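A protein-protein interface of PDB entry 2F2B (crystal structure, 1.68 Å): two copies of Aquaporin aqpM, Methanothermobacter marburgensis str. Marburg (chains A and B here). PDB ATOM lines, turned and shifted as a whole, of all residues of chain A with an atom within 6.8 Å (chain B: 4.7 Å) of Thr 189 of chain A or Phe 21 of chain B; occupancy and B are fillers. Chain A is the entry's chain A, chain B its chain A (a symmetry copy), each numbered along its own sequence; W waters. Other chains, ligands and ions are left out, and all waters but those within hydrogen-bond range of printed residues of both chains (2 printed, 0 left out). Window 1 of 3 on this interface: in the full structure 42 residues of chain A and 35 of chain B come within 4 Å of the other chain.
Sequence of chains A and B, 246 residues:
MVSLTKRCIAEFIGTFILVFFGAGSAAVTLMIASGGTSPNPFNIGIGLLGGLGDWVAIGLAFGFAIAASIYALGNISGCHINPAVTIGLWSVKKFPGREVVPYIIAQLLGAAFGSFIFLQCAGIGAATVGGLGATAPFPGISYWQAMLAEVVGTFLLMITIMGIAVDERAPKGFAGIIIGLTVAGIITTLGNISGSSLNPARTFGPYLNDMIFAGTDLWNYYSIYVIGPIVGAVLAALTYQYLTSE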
ATOM      1  N   LEU A  52     -22.742 -10.332  11.693  1.00  0.00           N
ATOM      2  CA  LEU A  52     -21.562 -11.192  11.710  1.00  0.00           C
ATOM      3  C   LEU A  52     -20.496 -10.544  12.590  1.00  0.00           C
ATOM      4  O   LEU A  52     -19.525 -11.194  12.982  1.00  0.00           O
ATOM      5  CB  LEU A  52     -21.017 -11.423  10.293  1.00  0.00           C
ATOM      6  CG  LEU A  52     -20.073 -12.633  10.191  1.00  0.00           C
ATOM      7  CD1 LEU A  52     -20.886 -13.918  10.341  1.00  0.00           C
ATOM      8  CD2 LEU A  52     -19.335 -12.626   8.850  1.00  0.00           C
ATOM      9  N   TRP A  55     -20.144 -12.400  15.676  1.00  0.00           N
ATOM     10  CA  TRP A  55     -19.388 -13.629  15.527  1.00  0.00           C
ATOM     11  C   TRP A  55     -17.884 -13.414  15.460  1.00  0.00           C
ATOM     12  O   TRP A  55     -17.130 -14.195  16.036  1.00  0.00           O
ATOM     13  CB  TRP A  55     -19.875 -14.412  14.304  1.00  0.00           C
ATOM     14  CG  TRP A  55     -21.087 -15.254  14.616  1.00  0.00           C
ATOM     15  CD1 TRP A  55     -22.336 -15.140  14.072  1.00  0.00           C
ATOM     16  CD2 TRP A  55     -21.156 -16.336  15.555  1.00  0.00           C
ATOM     17  NE1 TRP A  55     -23.177 -16.087  14.613  1.00  0.00           N
ATOM     18  CE2 TRP A  55     -22.477 -16.834  15.524  1.00  0.00           C
ATOM     19  CE3 TRP A  55     -20.227 -16.932  16.418  1.00  0.00           C
ATOM     20  CZ2 TRP A  55     -22.895 -17.903  16.327  1.00  0.00           C
ATOM     21  CZ3 TRP A  55     -20.642 -17.993  17.219  1.00  0.00           C
ATOM     22  CH2 TRP A  55     -21.968 -18.468  17.164  1.00  0.00           C
ATOM     23  N   ALA A 149     -18.808 -29.832   9.876  1.00  0.00           N
ATOM     24  CA  ALA A 149     -18.274 -28.503  10.168  1.00  0.00           C
ATOM     25  C   ALA A 149     -17.084 -28.591  11.121  1.00  0.00           C
ATOM     26  O   ALA A 149     -16.056 -27.939  10.910  1.00  0.00           O
ATOM     27  CB  ALA A 149     -19.367 -27.619  10.773  1.00  0.00           C
ATOM     28  N   VAL A 152     -13.927 -30.025   9.234  1.00  0.00           N
ATOM     29  CA  VAL A 152     -13.277 -29.042   8.364  1.00  0.00           C
ATOM     30  C   VAL A 152     -12.613 -27.935   9.182  1.00  0.00           C
ATOM     31  O   VAL A 152     -11.475 -27.543   8.911  1.00  0.00           O
ATOM     32  CB  VAL A 152     -14.290 -28.418   7.370  1.00  0.00           C
ATOM     33  CG1 VAL A 152     -13.579 -27.415   6.454  1.00  0.00           C
ATOM     34  CG2 VAL A 152     -14.938 -29.521   6.533  1.00  0.00           C
ATOM     35  N   GLY A 153     -13.323 -27.436  10.187  1.00  0.00           N
ATOM     36  CA  GLY A 153     -12.766 -26.388  11.025  1.00  0.00           C
ATOM     37  C   GLY A 153     -11.513 -26.828  11.766  1.00  0.00           C
ATOM     38  O   GLY A 153     -10.515 -26.110  11.790  1.00  0.00           O
ATOM     39  N   THR A 154     -11.544 -28.015  12.365  1.00  0.00           N
ATOM     40  CA  THR A 154     -10.381 -28.480  13.107  1.00  0.00           C
ATOM     41  C   THR A 154      -9.242 -28.856  12.161  1.00  0.00           C
ATOM     42  O   THR A 154      -8.073 -28.799  12.538  1.00  0.00           O
ATOM     43  CB  THR A 154     -10.740 -29.671  14.021  1.00  0.00           C
ATOM     44  OG1 THR A 154     -11.926 -29.356  14.768  1.00  0.00           O
ATOM     45  CG2 THR A 154      -9.610 -29.932  15.012  1.00  0.00           C
ATOM     46  N   LEU A 156      -8.398 -27.172   9.461  1.00  0.00           N
ATOM     47  CA  LEU A 156      -7.672 -25.924   9.219  1.00  0.00           C
ATOM     48  C   LEU A 156      -6.816 -25.555  10.425  1.00  0.00           C
ATOM     49  O   LEU A 156      -5.651 -25.179  10.280  1.00  0.00           O
ATOM     50  CB  LEU A 156      -8.636 -24.772   8.907  1.00  0.00           C
ATOM     51  CG  LEU A 156      -7.940 -23.413   8.728  1.00  0.00           C
ATOM     52  CD1 LEU A 156      -6.913 -23.506   7.603  1.00  0.00           C
ATOM     53  CD2 LEU A 156      -8.966 -22.330   8.423  1.00  0.00           C
ATOM     54  N   LEU A 157      -7.396 -25.657  11.618  1.00  0.00           N
ATOM     55  CA  LEU A 157      -6.657 -25.339  12.836  1.00  0.00           C
ATOM     56  C   LEU A 157      -5.387 -26.178  12.951  1.00  0.00           C
ATOM     57  O   LEU A 157      -4.295 -25.643  13.144  1.00  0.00           O
ATOM     58  CB  LEU A 157      -7.530 -25.579  14.073  1.00  0.00           C
ATOM     59  CG  LEU A 157      -6.810 -25.520  15.430  1.00  0.00           C
ATOM     60  CD1 LEU A 157      -6.130 -24.161  15.610  1.00  0.00           C
ATOM     61  CD2 LEU A 157      -7.811 -25.771  16.552  1.00  0.00           C
ATOM     62  N   THR A 182      -6.423 -17.704  13.485  1.00  0.00           N
ATOM     63  CA  THR A 182      -7.015 -18.747  12.655  1.00  0.00           C
ATOM     64  C   THR A 182      -8.300 -19.240  13.326  1.00  0.00           C
ATOM     65  O   THR A 182      -9.320 -19.435  12.668  1.00  0.00           O
ATOM     66  CB  THR A 182      -6.031 -19.908  12.452  1.00  0.00           C
ATOM     67  OG1 THR A 182      -4.881 -19.422  11.751  1.00  0.00           O
ATOM     68  CG2 THR A 182      -6.671 -21.022  11.626  1.00  0.00           C
ATOM     69  N   ALA A 184     -10.142 -17.521  15.390  1.00  0.00           N
ATOM     70  CA  ALA A 184     -11.122 -16.434  15.291  1.00  0.00           C
ATOM     71  C   ALA A 184     -11.846 -16.499  13.947  1.00  0.00           C
ATOM     72  O   ALA A 184     -13.067 -16.332  13.878  1.00  0.00           O
ATOM     73  CB  ALA A 184     -10.433 -15.071  15.453  1.00  0.00           C
ATOM     74  N   GLY A 185     -11.088 -16.754  12.883  1.00  0.00           N
ATOM     75  CA  GLY A 185     -11.674 -16.843  11.553  1.00  0.00           C
ATOM     76  C   GLY A 185     -12.598 -18.034  11.382  1.00  0.00           C
ATOM     77  O   GLY A 185     -13.650 -17.928  10.754  1.00  0.00           O
ATOM     78  N   ILE A 186     -12.209 -19.175  11.934  1.00  0.00           N
ATOM     79  CA  ILE A 186     -13.023 -20.381  11.840  1.00  0.00           C
ATOM     80  C   ILE A 186     -14.344 -20.177  12.585  1.00  0.00           C
ATOM     81  O   ILE A 186     -15.405 -20.565  12.093  1.00  0.00           O
ATOM     82  CB  ILE A 186     -12.255 -21.606  12.411  1.00  0.00           C
ATOM     83  CG1 ILE A 186     -11.033 -21.890  11.529  1.00  0.00           C
ATOM     84  CG2 ILE A 186     -13.171 -22.846  12.450  1.00  0.00           C
ATOM     85  CD1 ILE A 186     -10.013 -22.843  12.153  1.00  0.00           C
ATOM     86  N   ILE A 187     -14.285 -19.548  13.755  1.00  0.00           N
ATOM     87  CA  ILE A 187     -15.497 -19.297  14.535  1.00  0.00           C
ATOM     88  C   ILE A 187     -16.418 -18.319  13.802  1.00  0.00           C
ATOM     89  O   ILE A 187     -17.643 -18.461  13.826  1.00  0.00           O
ATOM     90  CB  ILE A 187     -15.146 -18.736  15.945  1.00  0.00           C
ATOM     91  CG1 ILE A 187     -14.529 -19.850  16.796  1.00  0.00           C
ATOM     92  CG2 ILE A 187     -16.397 -18.164  16.627  1.00  0.00           C
ATOM     93  CD1 ILE A 187     -13.908 -19.363  18.107  1.00  0.00           C
ATOM     94  N   THR A 188     -15.832 -17.328  13.142  1.00  0.00           N
ATOM     95  CA  THR A 188     -16.635 -16.353  12.416  1.00  0.00           C
ATOM     96  C   THR A 188     -17.500 -17.052  11.364  1.00  0.00           C
ATOM     97  O   THR A 188     -18.674 -16.720  11.191  1.00  0.00           O
ATOM     98  CB  THR A 188     -15.729 -15.293  11.744  1.00  0.00           C
ATOM     99  OG1 THR A 188     -14.941 -14.646  12.749  1.00  0.00           O
ATOM    100  CG2 THR A 188     -16.566 -14.242  11.019  1.00  0.00           C
ATOM    101  N   THR A 189     -16.926 -18.040  10.685  1.00  0.00           N
ATOM    102  CA  THR A 189     -17.649 -18.771   9.646  1.00  0.00           C
ATOM    103  C   THR A 189     -18.579 -19.870  10.168  1.00  0.00           C
ATOM    104  O   THR A 189     -19.753 -19.932   9.799  1.00  0.00           O
ATOM    105  CB  THR A 189     -16.668 -19.442   8.655  1.00  0.00           C
ATOM    106  OG1 THR A 189     -15.810 -18.449   8.074  1.00  0.00           O
ATOM    107  CG2 THR A 189     -17.437 -20.151   7.532  1.00  0.00           C
ATOM    108  N   LEU A 190     -18.040 -20.724  11.031  1.00  0.00           N
ATOM    109  CA  LEU A 190     -18.769 -21.880  11.562  1.00  0.00           C
ATOM    110  C   LEU A 190     -19.537 -21.715  12.875  1.00  0.00           C
ATOM    111  O   LEU A 190     -20.260 -22.626  13.285  1.00  0.00           O
ATOM    112  CB  LEU A 190     -17.784 -23.050  11.702  1.00  0.00           C
ATOM    113  CG  LEU A 190     -17.650 -24.123  10.608  1.00  0.00           C
ATOM    114  CD1 LEU A 190     -18.163 -23.636   9.272  1.00  0.00           C
ATOM    115  CD2 LEU A 190     -16.202 -24.573  10.526  1.00  0.00           C
ATOM    116  N   GLY A 191     -19.389 -20.570  13.529  1.00  0.00           N
ATOM    117  CA  GLY A 191     -20.075 -20.359  14.792  1.00  0.00           C
ATOM    118  C   GLY A 191     -21.573 -20.605  14.733  1.00  0.00           C
ATOM    119  O   GLY A 191     -22.126 -21.305  15.585  1.00  0.00           O
ATOM    120  N   ASN A 192     -22.229 -20.048  13.721  1.00  0.00           N
ATOM    121  CA  ASN A 192     -23.676 -20.189  13.587  1.00  0.00           C
ATOM    122  C   ASN A 192     -24.119 -21.508  12.956  1.00  0.00           C
ATOM    123  O   ASN A 192     -25.290 -21.674  12.603  1.00  0.00           O
ATOM    124  CB  ASN A 192     -24.249 -19.019  12.785  1.00  0.00           C
ATOM    125  CG  ASN A 192     -25.575 -18.526  13.343  1.00  0.00           C
ATOM    126  OD1 ASN A 192     -25.617 -17.571  14.114  1.00  0.00           O
ATOM    127  ND2 ASN A 192     -26.663 -19.190  12.967  1.00  0.00           N
ATOM    128  N   ILE A 193     -23.187 -22.443  12.810  1.00  0.00           N
ATOM    129  CA  ILE A 193     -23.522 -23.750  12.257  1.00  0.00           C
ATOM    130  C   ILE A 193     -23.421 -24.807  13.355  1.00  0.00           C
ATOM    131  O   ILE A 193     -24.419 -25.437  13.711  1.00  0.00           O
ATOM    132  CB  ILE A 193     -22.596 -24.122  11.070  1.00  0.00           C
ATOM    133  CG1 ILE A 193     -22.836 -23.143   9.912  1.00  0.00           C
ATOM    134  CG2 ILE A 193     -22.883 -25.545  10.601  1.00  0.00           C
ATOM    135  CD1 ILE A 193     -21.965 -23.389   8.697  1.00  0.00           C
ATOM    136  N   SER A 196     -18.757 -23.991  16.373  1.00  0.00           N
ATOM    137  CA  SER A 196     -17.319 -23.989  16.083  1.00  0.00           C
ATOM    138  C   SER A 196     -16.435 -24.258  17.297  1.00  0.00           C
ATOM    139  O   SER A 196     -15.620 -23.416  17.689  1.00  0.00           O
ATOM    140  CB  SER A 196     -16.916 -22.657  15.441  1.00  0.00           C
ATOM    141  OG  SER A 196     -15.546 -22.670  15.066  1.00  0.00           O
ATOM    142  N   ILE B  17      -9.992 -23.942   1.279  1.00  0.00           N
ATOM    143  CA  ILE B  17     -10.077 -23.229   2.555  1.00  0.00           C
ATOM    144  C   ILE B  17     -10.542 -21.791   2.357  1.00  0.00           C
ATOM    145  O   ILE B  17     -11.432 -21.304   3.066  1.00  0.00           O
ATOM    146  CB  ILE B  17      -8.704 -23.236   3.273  1.00  0.00           C
ATOM    147  CG1 ILE B  17      -8.408 -24.651   3.784  1.00  0.00           C
ATOM    148  CG2 ILE B  17      -8.698 -22.220   4.424  1.00  0.00           C
ATOM    149  CD1 ILE B  17      -6.969 -24.870   4.226  1.00  0.00           C
ATOM    150  N   LEU B  18      -9.939 -21.117   1.387  1.00  0.00           N
ATOM    151  CA  LEU B  18     -10.287 -19.732   1.088  1.00  0.00           C
ATOM    152  C   LEU B  18     -11.788 -19.570   0.825  1.00  0.00           C
ATOM    153  O   LEU B  18     -12.435 -18.691   1.395  1.00  0.00           O
ATOM    154  CB  LEU B  18      -9.472 -19.257  -0.124  1.00  0.00           C
ATOM    155  CG  LEU B  18      -9.566 -17.790  -0.555  1.00  0.00           C
ATOM    156  CD1 LEU B  18      -8.310 -17.408  -1.338  1.00  0.00           C
ATOM    157  CD2 LEU B  18     -10.811 -17.577  -1.394  1.00  0.00           C
ATOM    158  N   VAL B  19     -12.341 -20.430  -0.025  1.00  0.00           N
ATOM    159  CA  VAL B  19     -13.757 -20.358  -0.372  1.00  0.00           C
ATOM    160  C   VAL B  19     -14.698 -20.868   0.720  1.00  0.00           C
ATOM    161  O   VAL B  19     -15.725 -20.246   1.004  1.00  0.00           O
ATOM    162  CB  VAL B  19     -14.024 -21.122  -1.693  1.00  0.00           C
ATOM    163  CG1 VAL B  19     -15.509 -21.099  -2.032  1.00  0.00           C
ATOM    164  CG2 VAL B  19     -13.219 -20.476  -2.820  1.00  0.00           C
ATOM    165  N   PHE B  20     -14.358 -21.996   1.333  1.00  0.00           N
ATOM    166  CA  PHE B  20     -15.196 -22.549   2.392  1.00  0.00           C
ATOM    167  C   PHE B  20     -15.394 -21.538   3.524  1.00  0.00           C
ATOM    168  O   PHE B  20     -16.520 -21.233   3.907  1.00  0.00           O
ATOM    169  CB  PHE B  20     -14.569 -23.843   2.939  1.00  0.00           C
ATOM    170  CG  PHE B  20     -15.372 -24.498   4.040  1.00  0.00           C
ATOM    171  CD1 PHE B  20     -15.324 -24.009   5.345  1.00  0.00           C
ATOM    172  CD2 PHE B  20     -16.180 -25.598   3.768  1.00  0.00           C
ATOM    173  CE1 PHE B  20     -16.068 -24.603   6.364  1.00  0.00           C
ATOM    174  CE2 PHE B  20     -16.931 -26.205   4.778  1.00  0.00           C
ATOM    175  CZ  PHE B  20     -16.875 -25.705   6.082  1.00  0.00           C
ATOM    176  N   PHE B  21     -14.296 -20.999   4.041  1.00  0.00           N
ATOM    177  CA  PHE B  21     -14.380 -20.053   5.148  1.00  0.00           C
ATOM    178  C   PHE B  21     -14.749 -18.623   4.769  1.00  0.00           C
ATOM    179  O   PHE B  21     -15.603 -18.012   5.417  1.00  0.00           O
ATOM    180  CB  PHE B  21     -13.065 -20.082   5.932  1.00  0.00           C
ATOM    181  CG  PHE B  21     -12.855 -21.366   6.681  1.00  0.00           C
ATOM    182  CD1 PHE B  21     -13.508 -21.591   7.892  1.00  0.00           C
ATOM    183  CD2 PHE B  21     -12.074 -22.384   6.141  1.00  0.00           C
ATOM    184  CE1 PHE B  21     -13.390 -22.817   8.550  1.00  0.00           C
ATOM    185  CE2 PHE B  21     -11.951 -23.612   6.791  1.00  0.00           C
ATOM    186  CZ  PHE B  21     -12.613 -23.826   8.000  1.00  0.00           C
ATOM    187  N   GLY B  22     -14.123 -18.093   3.721  1.00  0.00           N
ATOM    188  CA  GLY B  22     -14.416 -16.732   3.302  1.00  0.00           C
ATOM    189  C   GLY B  22     -15.806 -16.545   2.720  1.00  0.00           C
ATOM    190  O   GLY B  22     -16.624 -15.794   3.259  1.00  0.00           O
ATOM    191  N   ALA B  23     -16.081 -17.218   1.608  1.00  0.00           N
ATOM    192  CA  ALA B  23     -17.387 -17.101   0.969  1.00  0.00           C
ATOM    193  C   ALA B  23     -18.464 -17.621   1.913  1.00  0.00           C
ATOM    194  O   ALA B  23     -19.609 -17.162   1.885  1.00  0.00           O
ATOM    195  CB  ALA B  23     -17.403 -17.884  -0.343  1.00  0.00           C
ATOM    196  N   GLY B  24     -18.089 -18.580   2.756  1.00  0.00           N
ATOM    197  CA  GLY B  24     -19.036 -19.138   3.704  1.00  0.00           C
ATOM    198  C   GLY B  24     -19.527 -18.113   4.710  1.00  0.00           C
ATOM    199  O   GLY B  24     -20.712 -18.095   5.057  1.00  0.00           O
ATOM    200  N   SER B  25     -18.632 -17.245   5.176  1.00  0.00           N
ATOM    201  CA  SER B  25     -19.020 -16.230   6.152  1.00  0.00           C
ATOM    202  C   SER B  25     -20.040 -15.257   5.566  1.00  0.00           C
ATOM    203  O   SER B  25     -20.922 -14.777   6.278  1.00  0.00           O
ATOM    204  CB  SER B  25     -17.792 -15.456   6.650  1.00  0.00           C
ATOM    205  OG  SER B  25     -17.251 -14.618   5.640  1.00  0.00           O
ATOM    206  N   VAL B  28     -23.410 -16.991   5.532  1.00  0.00           N
ATOM    207  CA  VAL B  28     -23.942 -17.020   6.892  1.00  0.00           C
ATOM    208  C   VAL B  28     -24.538 -15.671   7.292  1.00  0.00           C
ATOM    209  O   VAL B  28     -25.592 -15.615   7.919  1.00  0.00           O
ATOM    210  CB  VAL B  28     -22.849 -17.407   7.919  1.00  0.00           C
ATOM    211  CG1 VAL B  28     -23.368 -17.211   9.337  1.00  0.00           C
ATOM    212  CG2 VAL B  28     -22.438 -18.858   7.713  1.00  0.00           C
ATOM    213  N   ALA B  61     -12.839 -13.145   7.873  1.00  0.00           N
ATOM    214  CA  ALA B  61     -13.037 -14.584   7.737  1.00  0.00           C
ATOM    215  C   ALA B  61     -12.151 -15.013   6.562  1.00  0.00           C
ATOM    216  O   ALA B  61     -11.515 -16.069   6.594  1.00  0.00           O
ATOM    217  CB  ALA B  61     -14.509 -14.902   7.455  1.00  0.00           C
ATOM    218  N   ALA B  65      -8.269 -16.908   7.163  1.00  0.00           N
ATOM    219  CA  ALA B  65      -8.163 -18.200   6.493  1.00  0.00           C
ATOM    220  C   ALA B  65      -7.002 -18.158   5.496  1.00  0.00           C
ATOM    221  O   ALA B  65      -6.281 -19.145   5.323  1.00  0.00           O
ATOM    222  CB  ALA B  65      -9.472 -18.539   5.779  1.00  0.00           C
ATOM    223  N   PHE B 118     -19.109 -26.605   1.876  1.00  0.00           N
ATOM    224  CA  PHE B 118     -19.716 -25.642   2.787  1.00  0.00           C
ATOM    225  C   PHE B 118     -21.236 -25.769   2.686  1.00  0.00           C
ATOM    226  O   PHE B 118     -21.949 -25.724   3.691  1.00  0.00           O
ATOM    227  CB  PHE B 118     -19.321 -24.208   2.447  1.00  0.00           C
ATOM    228  CG  PHE B 118     -19.911 -23.205   3.387  1.00  0.00           C
ATOM    229  CD1 PHE B 118     -19.370 -23.026   4.656  1.00  0.00           C
ATOM    230  CD2 PHE B 118     -21.068 -22.513   3.047  1.00  0.00           C
ATOM    231  CE1 PHE B 118     -19.979 -22.175   5.580  1.00  0.00           C
ATOM    232  CE2 PHE B 118     -21.683 -21.662   3.962  1.00  0.00           C
ATOM    233  CZ  PHE B 118     -21.138 -21.496   5.231  1.00  0.00           C
HETATM  234  O   HOH W   1      -9.249 -18.697   9.793  1.00  0.00           O
HETATM  235  O   HOH W   2     -11.783 -17.969   8.460  1.00  0.00           O
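Of the 13 printed residues of chain B, 7 touch a printed residue of chain A. Of the 20 printed residues of chain A, 9 touch a printed residue of chain B. Hydrophobic or aromatic side chains of chain A within 4 Å of the printed part of chain B: Leu 52, Val 152, Leu 156, Ile 186, Leu 190 and Ile 193. Among the printed residues, 17 pairs touch across the chains. Among the printed residues, no Asp or Glu carboxylate lies within 4 Å of a Lys or Arg side-chain nitrogen of the other chain.
Water W2 bridges O of Ala 61 of chain B (2.7 Å) and O of Gly 185 of chain A (3.0 Å). Water W1 lies within hydrogen-bond range of the backbone carbonyl oxygen (O) of Thr 182 of chain A (3.0 Å) and the backbone NH (N) of Ala 65 of chain B (3.3 Å).
Val 152 of chain A touches Phe 20 of chain B (CG1 to CZ, 3.7 Å). Gly 153 of chain A touches Phe 21 of chain B (CA to CZ, 3.97 Å). CD2 of Leu 156 of chain A touches CE2 of Phe 21 of chain B (3.6 Å). Ile 186 of chain A touches Phe 21 of chain B. CB of Ser 25 of chain B touches OG1 of Thr 189 of chain A, at 3.9 Å. Thr 189 of chain A touches Ala 61 of chain B (OG1 to CB, 3.8 Å). Leu 190 of chain A touches Phe 20 of chain B (CD1 to CE1, 3.7 Å). Leu 190 of chain A touches Phe 21 of chain B. Asn 192 of chain A touches Val 28 of chain B. Ile 193 of chain A touches Phe 118 of chain B (CD1 to CE1, 3.9 Å).
The indole nitrogen (NE1) of Trp 55 of chain A is in hydrogen-bond range of the side-chain amide oxygen (OD1) of Asn 192 of chain A, 2.9 Å away. O of Gly 185 of chain A sits at hydrogen-bond distance from OG1 of Thr 189 of chain A. The side-chain hydroxyl (OG) of Ser 25 of chain B lies within hydrogen-bond range of the backbone carbonyl oxygen (O) of Gly 22 of chain B (2.7 Å).
No position is printed for both chains.
Of chain B, only Phe 20 (3.9 Å), Phe 21 (2.7 Å), Ser 25 (3.9 Å), Val 28 (3.6 Å), Ala 61 (3.8 Å) and Phe 118 (3.8 Å) come within 4 Å of Thr 189 of chain A. Printed residues of chain A within 4 Å of Ser 25 of chain B: Leu 52 (3.7 Å) and Thr 189 (3.9 Å). Printed residues of chain B within 4 Å of Val 152 of chain A: Phe 20 (3.7 Å) and Phe 21 (3.99 Å). Of the printed residues of chain A, Phe 118 of chain B touches Thr 189 and Ile 193. Thr 154 of chain A touches none of the printed residues of chain B. The nearest residue of chain B that does not touch Thr 189 of chain A is Gly 24 of chain B (4.1 Å). The nearest printed residue of chain A that does not touch Phe 21 of chain B is Gly 185 of chain A (4.7 Å).
The backbone carbonyl oxygen (O) of Phe 21 of chain B lies within hydrogen-bond range of the side-chain hydroxyl (OG1) of Thr 189 of chain A, at 2.7 Å.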
